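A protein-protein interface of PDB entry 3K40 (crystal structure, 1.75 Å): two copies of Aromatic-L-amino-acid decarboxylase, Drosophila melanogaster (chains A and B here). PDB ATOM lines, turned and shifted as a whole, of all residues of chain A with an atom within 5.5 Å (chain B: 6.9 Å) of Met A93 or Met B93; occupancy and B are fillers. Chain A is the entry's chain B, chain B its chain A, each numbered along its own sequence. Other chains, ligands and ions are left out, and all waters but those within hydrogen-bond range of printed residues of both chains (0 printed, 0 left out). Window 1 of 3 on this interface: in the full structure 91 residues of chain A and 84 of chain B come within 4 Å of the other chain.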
ATOM      1  N   ALA A  10      -7.824   5.225 -23.288  1.00  0.00           N
ATOM      2  CA  ALA A  10      -9.077   5.501 -24.024  1.00  0.00           C
ATOM      3  C   ALA A  10      -8.833   6.643 -24.999  1.00  0.00           C
ATOM      4  O   ALA A  10      -9.301   6.621 -26.148  1.00  0.00           O
ATOM      5  CB  ALA A  10     -10.195   5.865 -23.094  1.00  0.00           C
ATOM      6  N   MET A  13      -7.036   5.466 -27.917  1.00  0.00           N
ATOM      7  CA  MET A  13      -7.961   4.704 -28.787  1.00  0.00           C
ATOM      8  C   MET A  13      -8.864   5.639 -29.606  1.00  0.00           C
ATOM      9  O   MET A  13      -9.203   5.355 -30.762  1.00  0.00           O
ATOM     10  CB  MET A  13      -8.806   3.728 -27.942  1.00  0.00           C
ATOM     11  CG  MET A  13      -9.714   2.868 -28.779  1.00  0.00           C
ATOM     12  SD  MET A  13      -8.790   1.796 -29.885  1.00  0.00           S
ATOM     13  CE  MET A  13      -8.432   0.431 -28.741  1.00  0.00           C
ATOM     14  N   VAL A  14      -9.249   6.782 -29.034  1.00  0.00           N
ATOM     15  CA  VAL A  14     -10.031   7.775 -29.781  1.00  0.00           C
ATOM     16  C   VAL A  14      -9.198   8.218 -30.990  1.00  0.00           C
ATOM     17  O   VAL A  14      -9.713   8.249 -32.115  1.00  0.00           O
ATOM     18  CB  VAL A  14     -10.380   9.004 -28.919  1.00  0.00           C
ATOM     19  CG1 VAL A  14     -10.972  10.128 -29.779  1.00  0.00           C
ATOM     20  CG2 VAL A  14     -11.384   8.621 -27.795  1.00  0.00           C
ATOM     21  N   ILE A  17      -9.165   5.345 -33.577  1.00  0.00           N
ATOM     22  CA  ILE A  17     -10.431   5.205 -34.299  1.00  0.00           C
ATOM     23  C   ILE A  17     -10.589   6.287 -35.394  1.00  0.00           C
ATOM     24  O   ILE A  17     -10.949   5.974 -36.543  1.00  0.00           O
ATOM     25  CB  ILE A  17     -11.620   5.217 -33.309  1.00  0.00           C
ATOM     26  CG1 ILE A  17     -11.587   3.912 -32.488  1.00  0.00           C
ATOM     27  CG2 ILE A  17     -12.966   5.391 -34.052  1.00  0.00           C
ATOM     28  CD1 ILE A  17     -12.484   3.933 -31.234  1.00  0.00           C
ATOM     29  N   ALA A  88     -22.683   7.956 -32.272  1.00  0.00           N
ATOM     30  CA  ALA A  88     -23.095   6.678 -31.674  1.00  0.00           C
ATOM     31  C   ALA A  88     -21.937   6.048 -30.893  1.00  0.00           C
ATOM     32  O   ALA A  88     -22.154   5.447 -29.837  1.00  0.00           O
ATOM     33  CB  ALA A  88     -23.635   5.718 -32.752  1.00  0.00           C
ATOM     34  N   ILE A  89     -20.709   6.203 -31.384  1.00  0.00           N
ATOM     35  CA  ILE A  89     -19.533   5.674 -30.661  1.00  0.00           C
ATOM     36  C   ILE A  89     -19.479   6.310 -29.269  1.00  0.00           C
ATOM     37  O   ILE A  89     -19.281   5.640 -28.254  1.00  0.00           O
ATOM     38  CB  ILE A  89     -18.220   5.946 -31.436  1.00  0.00           C
ATOM     39  CG1 ILE A  89     -18.152   5.014 -32.671  1.00  0.00           C
ATOM     40  CG2 ILE A  89     -17.029   5.641 -30.560  1.00  0.00           C
ATOM     41  CD1 ILE A  89     -16.939   5.298 -33.647  1.00  0.00           C
ATOM     42  N   VAL A  90     -19.664   7.626 -29.222  1.00  0.00           N
ATOM     43  CA  VAL A  90     -19.548   8.339 -27.929  1.00  0.00           C
ATOM     44  C   VAL A  90     -20.704   7.949 -26.997  1.00  0.00           C
ATOM     45  O   VAL A  90     -20.470   7.735 -25.806  1.00  0.00           O
ATOM     46  CB  VAL A  90     -19.419   9.861 -28.124  1.00  0.00           C
ATOM     47  CG1 VAL A  90     -19.175  10.555 -26.756  1.00  0.00           C
ATOM     48  CG2 VAL A  90     -18.193  10.150 -29.006  1.00  0.00           C
ATOM     49  N   ALA A  91     -21.923   7.835 -27.523  1.00  0.00           N
ATOM     50  CA  ALA A  91     -23.050   7.369 -26.724  1.00  0.00           C
ATOM     51  C   ALA A  91     -22.731   6.003 -26.107  1.00  0.00           C
ATOM     52  O   ALA A  91     -22.950   5.770 -24.914  1.00  0.00           O
ATOM     53  CB  ALA A  91     -24.256   7.252 -27.580  1.00  0.00           C
ATOM     54  N   ASP A  92     -22.222   5.095 -26.923  1.00  0.00           N
ATOM     55  CA  ASP A  92     -21.948   3.741 -26.386  1.00  0.00           C
ATOM     56  C   ASP A  92     -20.873   3.671 -25.296  1.00  0.00           C
ATOM     57  O   ASP A  92     -20.895   2.749 -24.458  1.00  0.00           O
ATOM     58  CB  ASP A  92     -21.697   2.778 -27.529  1.00  0.00           C
ATOM     59  CG  ASP A  92     -23.039   2.209 -28.090  1.00  0.00           C
ATOM     60  OD1 ASP A  92     -24.080   2.316 -27.388  1.00  0.00           O
ATOM     61  OD2 ASP A  92     -23.048   1.684 -29.205  1.00  0.00           O
ATOM     62  N   MET A  93     -19.933   4.618 -25.291  1.00  0.00           N
ATOM     63  CA  MET A  93     -18.954   4.715 -24.194  1.00  0.00           C
ATOM     64  C   MET A  93     -19.688   4.922 -22.867  1.00  0.00           C
ATOM     65  O   MET A  93     -19.417   4.233 -21.870  1.00  0.00           O
ATOM     66  CB  MET A  93     -17.993   5.881 -24.428  1.00  0.00           C
ATOM     67  CG  MET A  93     -17.090   5.636 -25.605  1.00  0.00           C
ATOM     68  SD  MET A  93     -16.232   7.104 -26.299  1.00  0.00           S
ATOM     69  CE  MET A  93     -15.319   7.651 -24.885  1.00  0.00           C
ATOM     70  N   LEU A  94     -20.630   5.848 -22.896  1.00  0.00           N
ATOM     71  CA  LEU A  94     -21.412   6.168 -21.705  1.00  0.00           C
ATOM     72  C   LEU A  94     -22.349   5.046 -21.337  1.00  0.00           C
ATOM     73  O   LEU A  94     -22.434   4.678 -20.157  1.00  0.00           O
ATOM     74  CB  LEU A  94     -22.221   7.434 -21.937  1.00  0.00           C
ATOM     75  CG  LEU A  94     -22.995   7.854 -20.670  1.00  0.00           C
ATOM     76  CD1 LEU A  94     -22.107   7.873 -19.422  1.00  0.00           C
ATOM     77  CD2 LEU A  94     -23.652   9.208 -20.900  1.00  0.00           C
ATOM     78  N   SER A  95     -23.058   4.499 -22.337  1.00  0.00           N
ATOM     79  CA  SER A  95     -23.982   3.378 -22.075  1.00  0.00           C
ATOM     80  C   SER A  95     -23.232   2.221 -21.445  1.00  0.00           C
ATOM     81  O   SER A  95     -23.750   1.561 -20.542  1.00  0.00           O
ATOM     82  CB  SER A  95     -24.682   2.914 -23.358  1.00  0.00           C
ATOM     83  OG  SER A  95     -25.525   3.945 -23.812  1.00  0.00           O
ATOM     84  N   GLY A  96     -22.008   1.982 -21.910  1.00  0.00           N
ATOM     85  CA  GLY A  96     -21.180   0.888 -21.376  1.00  0.00           C
ATOM     86  C   GLY A  96     -20.923   1.064 -19.894  1.00  0.00           C
ATOM     87  O   GLY A  96     -20.991   0.087 -19.127  1.00  0.00           O
ATOM     88  N   ALA A  97     -20.684   2.317 -19.504  1.00  0.00           N
ATOM     89  CA  ALA A  97     -20.439   2.737 -18.123  1.00  0.00           C
ATOM     90  C   ALA A  97     -21.653   2.723 -17.194  1.00  0.00           C
ATOM     91  O   ALA A  97     -21.494   2.484 -15.993  1.00  0.00           O
ATOM     92  CB  ALA A  97     -19.804   4.112 -18.103  1.00  0.00           C
ATOM     93  N   PHE B   6     -15.429  14.920 -33.231  1.00  0.00           N
ATOM     94  CA  PHE B   6     -15.536  13.610 -32.563  1.00  0.00           C
ATOM     95  C   PHE B   6     -14.455  13.460 -31.505  1.00  0.00           C
ATOM     96  O   PHE B   6     -14.738  13.051 -30.366  1.00  0.00           O
ATOM     97  CB  PHE B   6     -15.406  12.485 -33.585  1.00  0.00           C
ATOM     98  CG  PHE B   6     -15.051  11.153 -32.989  1.00  0.00           C
ATOM     99  CD1 PHE B   6     -15.971  10.466 -32.168  1.00  0.00           C
ATOM    100  CD2 PHE B   6     -13.808  10.566 -33.248  1.00  0.00           C
ATOM    101  CE1 PHE B   6     -15.657   9.231 -31.637  1.00  0.00           C
ATOM    102  CE2 PHE B   6     -13.489   9.323 -32.702  1.00  0.00           C
ATOM    103  CZ  PHE B   6     -14.429   8.664 -31.872  1.00  0.00           C
ATOM    104  N   PHE B   9     -15.232  15.588 -28.398  1.00  0.00           N
ATOM    105  CA  PHE B   9     -16.417  14.988 -27.734  1.00  0.00           C
ATOM    106  C   PHE B   9     -16.051  13.688 -27.014  1.00  0.00           C
ATOM    107  O   PHE B   9     -16.324  13.515 -25.810  1.00  0.00           O
ATOM    108  CB  PHE B   9     -17.481  14.749 -28.790  1.00  0.00           C
ATOM    109  CG  PHE B   9     -18.827  14.261 -28.271  1.00  0.00           C
ATOM    110  CD1 PHE B   9     -19.249  14.522 -26.967  1.00  0.00           C
ATOM    111  CD2 PHE B   9     -19.698  13.594 -29.142  1.00  0.00           C
ATOM    112  CE1 PHE B   9     -20.497  14.116 -26.531  1.00  0.00           C
ATOM    113  CE2 PHE B   9     -20.971  13.168 -28.708  1.00  0.00           C
ATOM    114  CZ  PHE B   9     -21.370  13.448 -27.401  1.00  0.00           C
ATOM    115  N   ALA B  10     -15.450  12.771 -27.755  1.00  0.00           N
ATOM    116  CA  ALA B  10     -15.067  11.494 -27.175  1.00  0.00           C
ATOM    117  C   ALA B  10     -14.096  11.647 -25.999  1.00  0.00           C
ATOM    118  O   ALA B  10     -14.257  10.997 -24.961  1.00  0.00           O
ATOM    119  CB  ALA B  10     -14.512  10.560 -28.243  1.00  0.00           C
ATOM    120  N   LYS B  11     -13.117  12.545 -26.108  1.00  0.00           N
ATOM    121  CA  LYS B  11     -12.136  12.665 -25.033  1.00  0.00           C
ATOM    122  C   LYS B  11     -12.769  13.317 -23.780  1.00  0.00           C
ATOM    123  O   LYS B  11     -12.460  12.949 -22.653  1.00  0.00           O
ATOM    124  CB  LYS B  11     -10.908  13.436 -25.520  1.00  0.00           C
ATOM    125  CG  LYS B  11     -10.058  12.576 -26.490  1.00  0.00           C
ATOM    126  CD  LYS B  11      -8.889  13.353 -27.044  1.00  0.00           C
ATOM    127  CE  LYS B  11      -8.184  12.513 -28.135  1.00  0.00           C
ATOM    128  NZ  LYS B  11      -6.845  13.128 -28.504  1.00  0.00           N
ATOM    129  N   THR B  12     -13.672  14.255 -24.013  1.00  0.00           N
ATOM    130  CA  THR B  12     -14.503  14.822 -22.946  1.00  0.00           C
ATOM    131  C   THR B  12     -15.366  13.750 -22.244  1.00  0.00           C
ATOM    132  O   THR B  12     -15.529  13.763 -21.012  1.00  0.00           O
ATOM    133  CB  THR B  12     -15.355  15.951 -23.513  1.00  0.00           C
ATOM    134  OG1 THR B  12     -14.461  16.980 -23.987  1.00  0.00           O
ATOM    135  CG2 THR B  12     -16.319  16.522 -22.435  1.00  0.00           C
ATOM    136  N   MET B  13     -15.916  12.834 -23.027  1.00  0.00           N
ATOM    137  CA  MET B  13     -16.718  11.743 -22.470  1.00  0.00           C
ATOM    138  C   MET B  13     -15.841  10.786 -21.663  1.00  0.00           C
ATOM    139  O   MET B  13     -16.293  10.271 -20.655  1.00  0.00           O
ATOM    140  CB  MET B  13     -17.446  10.995 -23.591  1.00  0.00           C
ATOM    141  CG  MET B  13     -18.361   9.884 -23.064  1.00  0.00           C
ATOM    142  SD  MET B  13     -19.712  10.493 -22.015  1.00  0.00           S
ATOM    143  CE  MET B  13     -20.903  10.946 -23.270  1.00  0.00           C
ATOM    144  N   VAL B  14     -14.595  10.563 -22.099  1.00  0.00           N
ATOM    145  CA  VAL B  14     -13.615   9.794 -21.323  1.00  0.00           C
ATOM    146  C   VAL B  14     -13.441  10.440 -19.940  1.00  0.00           C
ATOM    147  O   VAL B  14     -13.539   9.752 -18.911  1.00  0.00           O
ATOM    148  CB  VAL B  14     -12.248   9.654 -22.031  1.00  0.00           C
ATOM    149  CG1 VAL B  14     -11.206   9.024 -21.117  1.00  0.00           C
ATOM    150  CG2 VAL B  14     -12.397   8.800 -23.281  1.00  0.00           C
ATOM    151  N   ASP B  15     -13.246  11.763 -19.921  1.00  0.00           N
ATOM    152  CA  ASP B  15     -13.136  12.487 -18.658  1.00  0.00           C
ATOM    153  C   ASP B  15     -14.395  12.279 -17.802  1.00  0.00           C
ATOM    154  O   ASP B  15     -14.292  12.013 -16.579  1.00  0.00           O
ATOM    155  CB  ASP B  15     -12.993  13.988 -18.941  1.00  0.00           C
ATOM    156  CG  ASP B  15     -11.672  14.346 -19.583  1.00  0.00           C
ATOM    157  OD1 ASP B  15     -10.681  13.590 -19.448  1.00  0.00           O
ATOM    158  OD2 ASP B  15     -11.628  15.435 -20.195  1.00  0.00           O
ATOM    159  N   ILE B  17     -16.679   9.854 -17.862  1.00  0.00           N
ATOM    160  CA  ILE B  17     -16.820   8.490 -17.356  1.00  0.00           C
ATOM    161  C   ILE B  17     -15.916   8.221 -16.148  1.00  0.00           C
ATOM    162  O   ILE B  17     -16.370   7.650 -15.117  1.00  0.00           O
ATOM    163  CB  ILE B  17     -16.583   7.485 -18.490  1.00  0.00           C
ATOM    164  CG1 ILE B  17     -17.762   7.562 -19.464  1.00  0.00           C
ATOM    165  CG2 ILE B  17     -16.379   6.059 -17.945  1.00  0.00           C
ATOM    166  CD1 ILE B  17     -17.500   6.840 -20.822  1.00  0.00           C
ATOM    167  N   ASN B  84     -18.375  -4.110 -15.296  1.00  0.00           N
ATOM    168  CA  ASN B  84     -17.855  -2.922 -15.911  1.00  0.00           C
ATOM    169  C   ASN B  84     -16.357  -2.951 -15.599  1.00  0.00           C
ATOM    170  O   ASN B  84     -15.938  -3.335 -14.491  1.00  0.00           O
ATOM    171  CB  ASN B  84     -18.537  -1.650 -15.334  1.00  0.00           C
ATOM    172  CG  ASN B  84     -17.783  -0.376 -15.689  1.00  0.00           C
ATOM    173  OD1 ASN B  84     -18.101   0.301 -16.681  1.00  0.00           O
ATOM    174  ND2 ASN B  84     -16.747  -0.070 -14.911  1.00  0.00           N
ATOM    175  N   ALA B  88     -12.502  -3.067 -20.744  1.00  0.00           N
ATOM    176  CA  ALA B  88     -13.631  -3.423 -21.626  1.00  0.00           C
ATOM    177  C   ALA B  88     -14.287  -2.208 -22.319  1.00  0.00           C
ATOM    178  O   ALA B  88     -14.697  -2.316 -23.484  1.00  0.00           O
ATOM    179  CB  ALA B  88     -14.663  -4.220 -20.847  1.00  0.00           C
ATOM    180  N   ILE B  89     -14.338  -1.061 -21.629  1.00  0.00           N
ATOM    181  CA  ILE B  89     -14.892   0.164 -22.224  1.00  0.00           C
ATOM    182  C   ILE B  89     -14.033   0.505 -23.459  1.00  0.00           C
ATOM    183  O   ILE B  89     -14.584   0.785 -24.512  1.00  0.00           O
ATOM    184  CB  ILE B  89     -14.853   1.337 -21.221  1.00  0.00           C
ATOM    185  CG1 ILE B  89     -15.900   1.076 -20.110  1.00  0.00           C
ATOM    186  CG2 ILE B  89     -15.102   2.669 -21.949  1.00  0.00           C
ATOM    187  CD1 ILE B  89     -15.801   2.008 -18.923  1.00  0.00           C
ATOM    188  N   VAL B  90     -12.704   0.436 -23.318  1.00  0.00           N
ATOM    189  CA  VAL B  90     -11.801   0.788 -24.431  1.00  0.00           C
ATOM    190  C   VAL B  90     -11.942  -0.186 -25.586  1.00  0.00           C
ATOM    191  O   VAL B  90     -11.998   0.233 -26.741  1.00  0.00           O
ATOM    192  CB  VAL B  90     -10.345   0.977 -24.005  1.00  0.00           C
ATOM    193  CG1 VAL B  90      -9.481   1.434 -25.220  1.00  0.00           C
ATOM    194  CG2 VAL B  90     -10.287   2.044 -22.932  1.00  0.00           C
ATOM    195  N   ALA B  91     -12.071  -1.477 -25.289  1.00  0.00           N
ATOM    196  CA  ALA B  91     -12.252  -2.443 -26.369  1.00  0.00           C
ATOM    197  C   ALA B  91     -13.526  -2.173 -27.122  1.00  0.00           C
ATOM    198  O   ALA B  91     -13.558  -2.307 -28.344  1.00  0.00           O
ATOM    199  CB  ALA B  91     -12.267  -3.858 -25.809  1.00  0.00           C
ATOM    200  N   ASP B  92     -14.591  -1.871 -26.399  1.00  0.00           N
ATOM    201  CA  ASP B  92     -15.892  -1.668 -27.043  1.00  0.00           C
ATOM    202  C   ASP B  92     -15.913  -0.427 -27.938  1.00  0.00           C
ATOM    203  O   ASP B  92     -16.669  -0.375 -28.915  1.00  0.00           O
ATOM    204  CB  ASP B  92     -17.012  -1.684 -26.017  1.00  0.00           C
ATOM    205  CG  ASP B  92     -17.496  -3.120 -25.733  1.00  0.00           C
ATOM    206  OD1 ASP B  92     -17.162  -4.051 -26.519  1.00  0.00           O
ATOM    207  OD2 ASP B  92     -18.217  -3.291 -24.753  1.00  0.00           O
ATOM    208  N   MET B  93     -15.074   0.555 -27.612  1.00  0.00           N
ATOM    209  CA  MET B  93     -14.891   1.726 -28.504  1.00  0.00           C
ATOM    210  C   MET B  93     -14.404   1.257 -29.875  1.00  0.00           C
ATOM    211  O   MET B  93     -14.912   1.691 -30.931  1.00  0.00           O
ATOM    212  CB  MET B  93     -13.870   2.673 -27.890  1.00  0.00           C
ATOM    213  CG  MET B  93     -14.441   3.396 -26.673  1.00  0.00           C
ATOM    214  SD  MET B  93     -13.167   4.252 -25.710  1.00  0.00           S
ATOM    215  CE  MET B  93     -12.813   5.565 -26.878  1.00  0.00           C
ATOM    216  N   LEU B  94     -13.409   0.380 -29.855  1.00  0.00           N
ATOM    217  CA  LEU B  94     -12.829  -0.167 -31.085  1.00  0.00           C
ATOM    218  C   LEU B  94     -13.824  -1.090 -31.801  1.00  0.00           C
ATOM    219  O   LEU B  94     -13.987  -0.964 -33.004  1.00  0.00           O
ATOM    220  CB  LEU B  94     -11.501  -0.892 -30.817  1.00  0.00           C
ATOM    221  CG  LEU B  94     -10.772  -1.441 -32.063  1.00  0.00           C
ATOM    222  CD1 LEU B  94     -10.672  -0.385 -33.189  1.00  0.00           C
ATOM    223  CD2 LEU B  94      -9.414  -2.037 -31.677  1.00  0.00           C
ATOM    224  N   SER B  95     -14.479  -2.000 -31.061  1.00  0.00           N
ATOM    225  CA  SER B  95     -15.507  -2.889 -31.646  1.00  0.00           C
ATOM    226  C   SER B  95     -16.607  -2.076 -32.298  1.00  0.00           C
ATOM    227  O   SER B  95     -17.133  -2.454 -33.352  1.00  0.00           O
ATOM    228  CB  SER B  95     -16.145  -3.754 -30.553  1.00  0.00           C
ATOM    229  OG  SER B  95     -15.156  -4.595 -30.055  1.00  0.00           O
ATOM    230  N   GLY B  96     -16.965  -0.970 -31.662  1.00  0.00           N
ATOM    231  CA  GLY B  96     -17.962  -0.055 -32.220  1.00  0.00           C
ATOM    232  C   GLY B  96     -17.602   0.402 -33.617  1.00  0.00           C
ATOM    233  O   GLY B  96     -18.481   0.472 -34.502  1.00  0.00           O
ATOM    234  N   ALA B  97     -16.313   0.658 -33.828  1.00  0.00           N
ATOM    235  CA  ALA B  97     -15.790   1.194 -35.094  1.00  0.00           C
ATOM    236  C   ALA B  97     -15.551   0.156 -36.187  1.00  0.00           C
ATOM    237  O   ALA B  97     -15.606   0.505 -37.367  1.00  0.00           O
ATOM    238  CB  ALA B  97     -14.490   1.973 -34.848  1.00  0.00           C
ATOM    239  N   ILE B  98     -15.257  -1.090 -35.805  1.00  0.00           N
ATOM    240  CA  ILE B  98     -14.863  -2.156 -36.748  1.00  0.00           C
ATOM    241  C   ILE B  98     -15.746  -3.418 -36.837  1.00  0.00           C
ATOM    242  O   ILE B  98     -15.619  -4.181 -37.787  1.00  0.00           O
ATOM    243  CB  ILE B  98     -13.378  -2.635 -36.566  1.00  0.00           C
ATOM    244  CG1 ILE B  98     -13.168  -3.399 -35.248  1.00  0.00           C
ATOM    245  CG2 ILE B  98     -12.386  -1.455 -36.752  1.00  0.00           C
ATOM    246  CD1 ILE B  98     -11.714  -3.888 -35.012  1.00  0.00           C
ATOM    247  N   ASN B 307     -17.547  -6.045 -19.777  1.00  0.00           N
ATOM    248  CA  ASN B 307     -18.821  -5.373 -20.076  1.00  0.00           C
ATOM    249  C   ASN B 307     -19.710  -6.207 -21.018  1.00  0.00           C
ATOM    250  O   ASN B 307     -19.217  -6.817 -21.969  1.00  0.00           O
ATOM    251  CB  ASN B 307     -18.618  -4.013 -20.768  1.00  0.00           C
ATOM    252  CG  ASN B 307     -17.755  -3.049 -19.996  1.00  0.00           C
ATOM    253  OD1 ASN B 307     -17.183  -3.371 -18.988  1.00  0.00           O
ATOM    254  ND2 ASN B 307     -17.632  -1.841 -20.533  1.00  0.00           N
ATOM    255  N   LEU B 357     -12.611  -9.137 -28.589  1.00  0.00           N
ATOM    256  CA  LEU B 357     -11.702  -8.022 -28.340  1.00  0.00           C
ATOM    257  C   LEU B 357     -11.741  -7.591 -26.869  1.00  0.00           C
ATOM    258  O   LEU B 357     -10.692  -7.452 -26.228  1.00  0.00           O
ATOM    259  CB  LEU B 357     -12.059  -6.841 -29.276  1.00  0.00           C
ATOM    260  CG  LEU B 357     -10.905  -5.872 -29.513  1.00  0.00           C
ATOM    261  CD1 LEU B 357      -9.829  -6.537 -30.358  1.00  0.00           C
ATOM    262  CD2 LEU B 357     -11.532  -4.653 -30.241  1.00  0.00           C
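Among the printed residues, pairs that only touch across the chains: Ile A17 with Met B93 (3.3 Å), Met A93 with Ile B17 (3.4 Å), Val A14 with Met B93 (3.5 Å), Met A93 with Ala B10 (3.5 Å), Met A93 with Val B14 (3.5 Å), Met A13 with Val B90 (3.6 Å), Met A93 with Met B93 (3.6 Å), Val A90 with Met B13 (3.6 Å), Ala A97 with Asn B84 (3.7 Å), Ala A10 with Val B14 (3.7 Å), Val A90 with Phe B9 (3.7 Å), Val A14 with Ala B10 (3.7 Å), Ala A10 with Met B93 (3.7 Å), Val A90 with Phe B6 (3.8 Å), Val A90 with Ala B10 (3.8 Å), Gly A96 with Asn B84 (3.8 Å), Ala A10 with Val B90 (3.8 Å), Ile A17 with Ala B97 (3.8 Å), Leu A94 with Ile B17 (3.9 Å), Ile A17 with Leu B94 (3.9 Å), Met A13 with Leu B94 (3.9 Å), Val A14 with Phe B6 (3.9 Å), Ala A97 with Ile B17 (3.9 Å), Leu A94 with Met B13 (3.96 Å) and Ile A89 with Phe B6 (3.99 Å).
Met A93 touches just these residues of chain B: Ala B10, Val B14, Ile B17 and Met B93. Met B93 touches just these residues of chain A: Ala A10, Val A14, Ile A17 and Met A93. Of the printed residues of chain B, Ile A89 touches Phe B6 (3.99 Å). Of the printed residues of chain A, Phe B9 touches Val A90 (3.7 Å). Printed residues of chain B within 4 Å of Met A13: Val B90 and Leu B94. Printed residues of chain A within 4 Å of Ala B97: Ile A17 (3.8 Å). The nearest residue of chain B that does not touch Met A93 is Met B13 (4.2 Å). The nearest printed residue of chain A that does not touch Ala B97 is Ile A89 (4.3 Å).
Printed residues of chain B that touch a printed residue of chain A: Phe B6, Phe B9, Ala B10, Met B13, Val B14, Ile B17, Asn B84, Val B90, Met B93, Leu B94 and Ala B97. Hydrophobic or aromatic side chains of chain B that line the printed part of chain A: Phe B6, Phe B9, Ala B10, Met B13, Val B14, Ile B17, Val B90, Met B93, Leu B94 and Ala B97. Of the 14 printed residues of chain A, 10 touch a printed residue of chain B. Printed residues of chain A that touch a printed residue of chain B: Ala A10, Met A13, Val A14, Ile A17, Ile A89, Val A90, Met A93, Leu A94, Gly A96 and Ala A97.
Ala A10 touches Val B14, and with the chains exchanged Val A14 touches Ala B10. Val A14 touches Met B93, and with the chains exchanged Met A93 touches Val B14. Ile A17 touches Met B93, and with the chains exchanged Met A93 touches Ile B17. Met A93 touches its own counterpart, Met B93. Of the 25 pairs that touch across the chains among the printed residues, 19 have their exchanged pair printed and touching as well.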
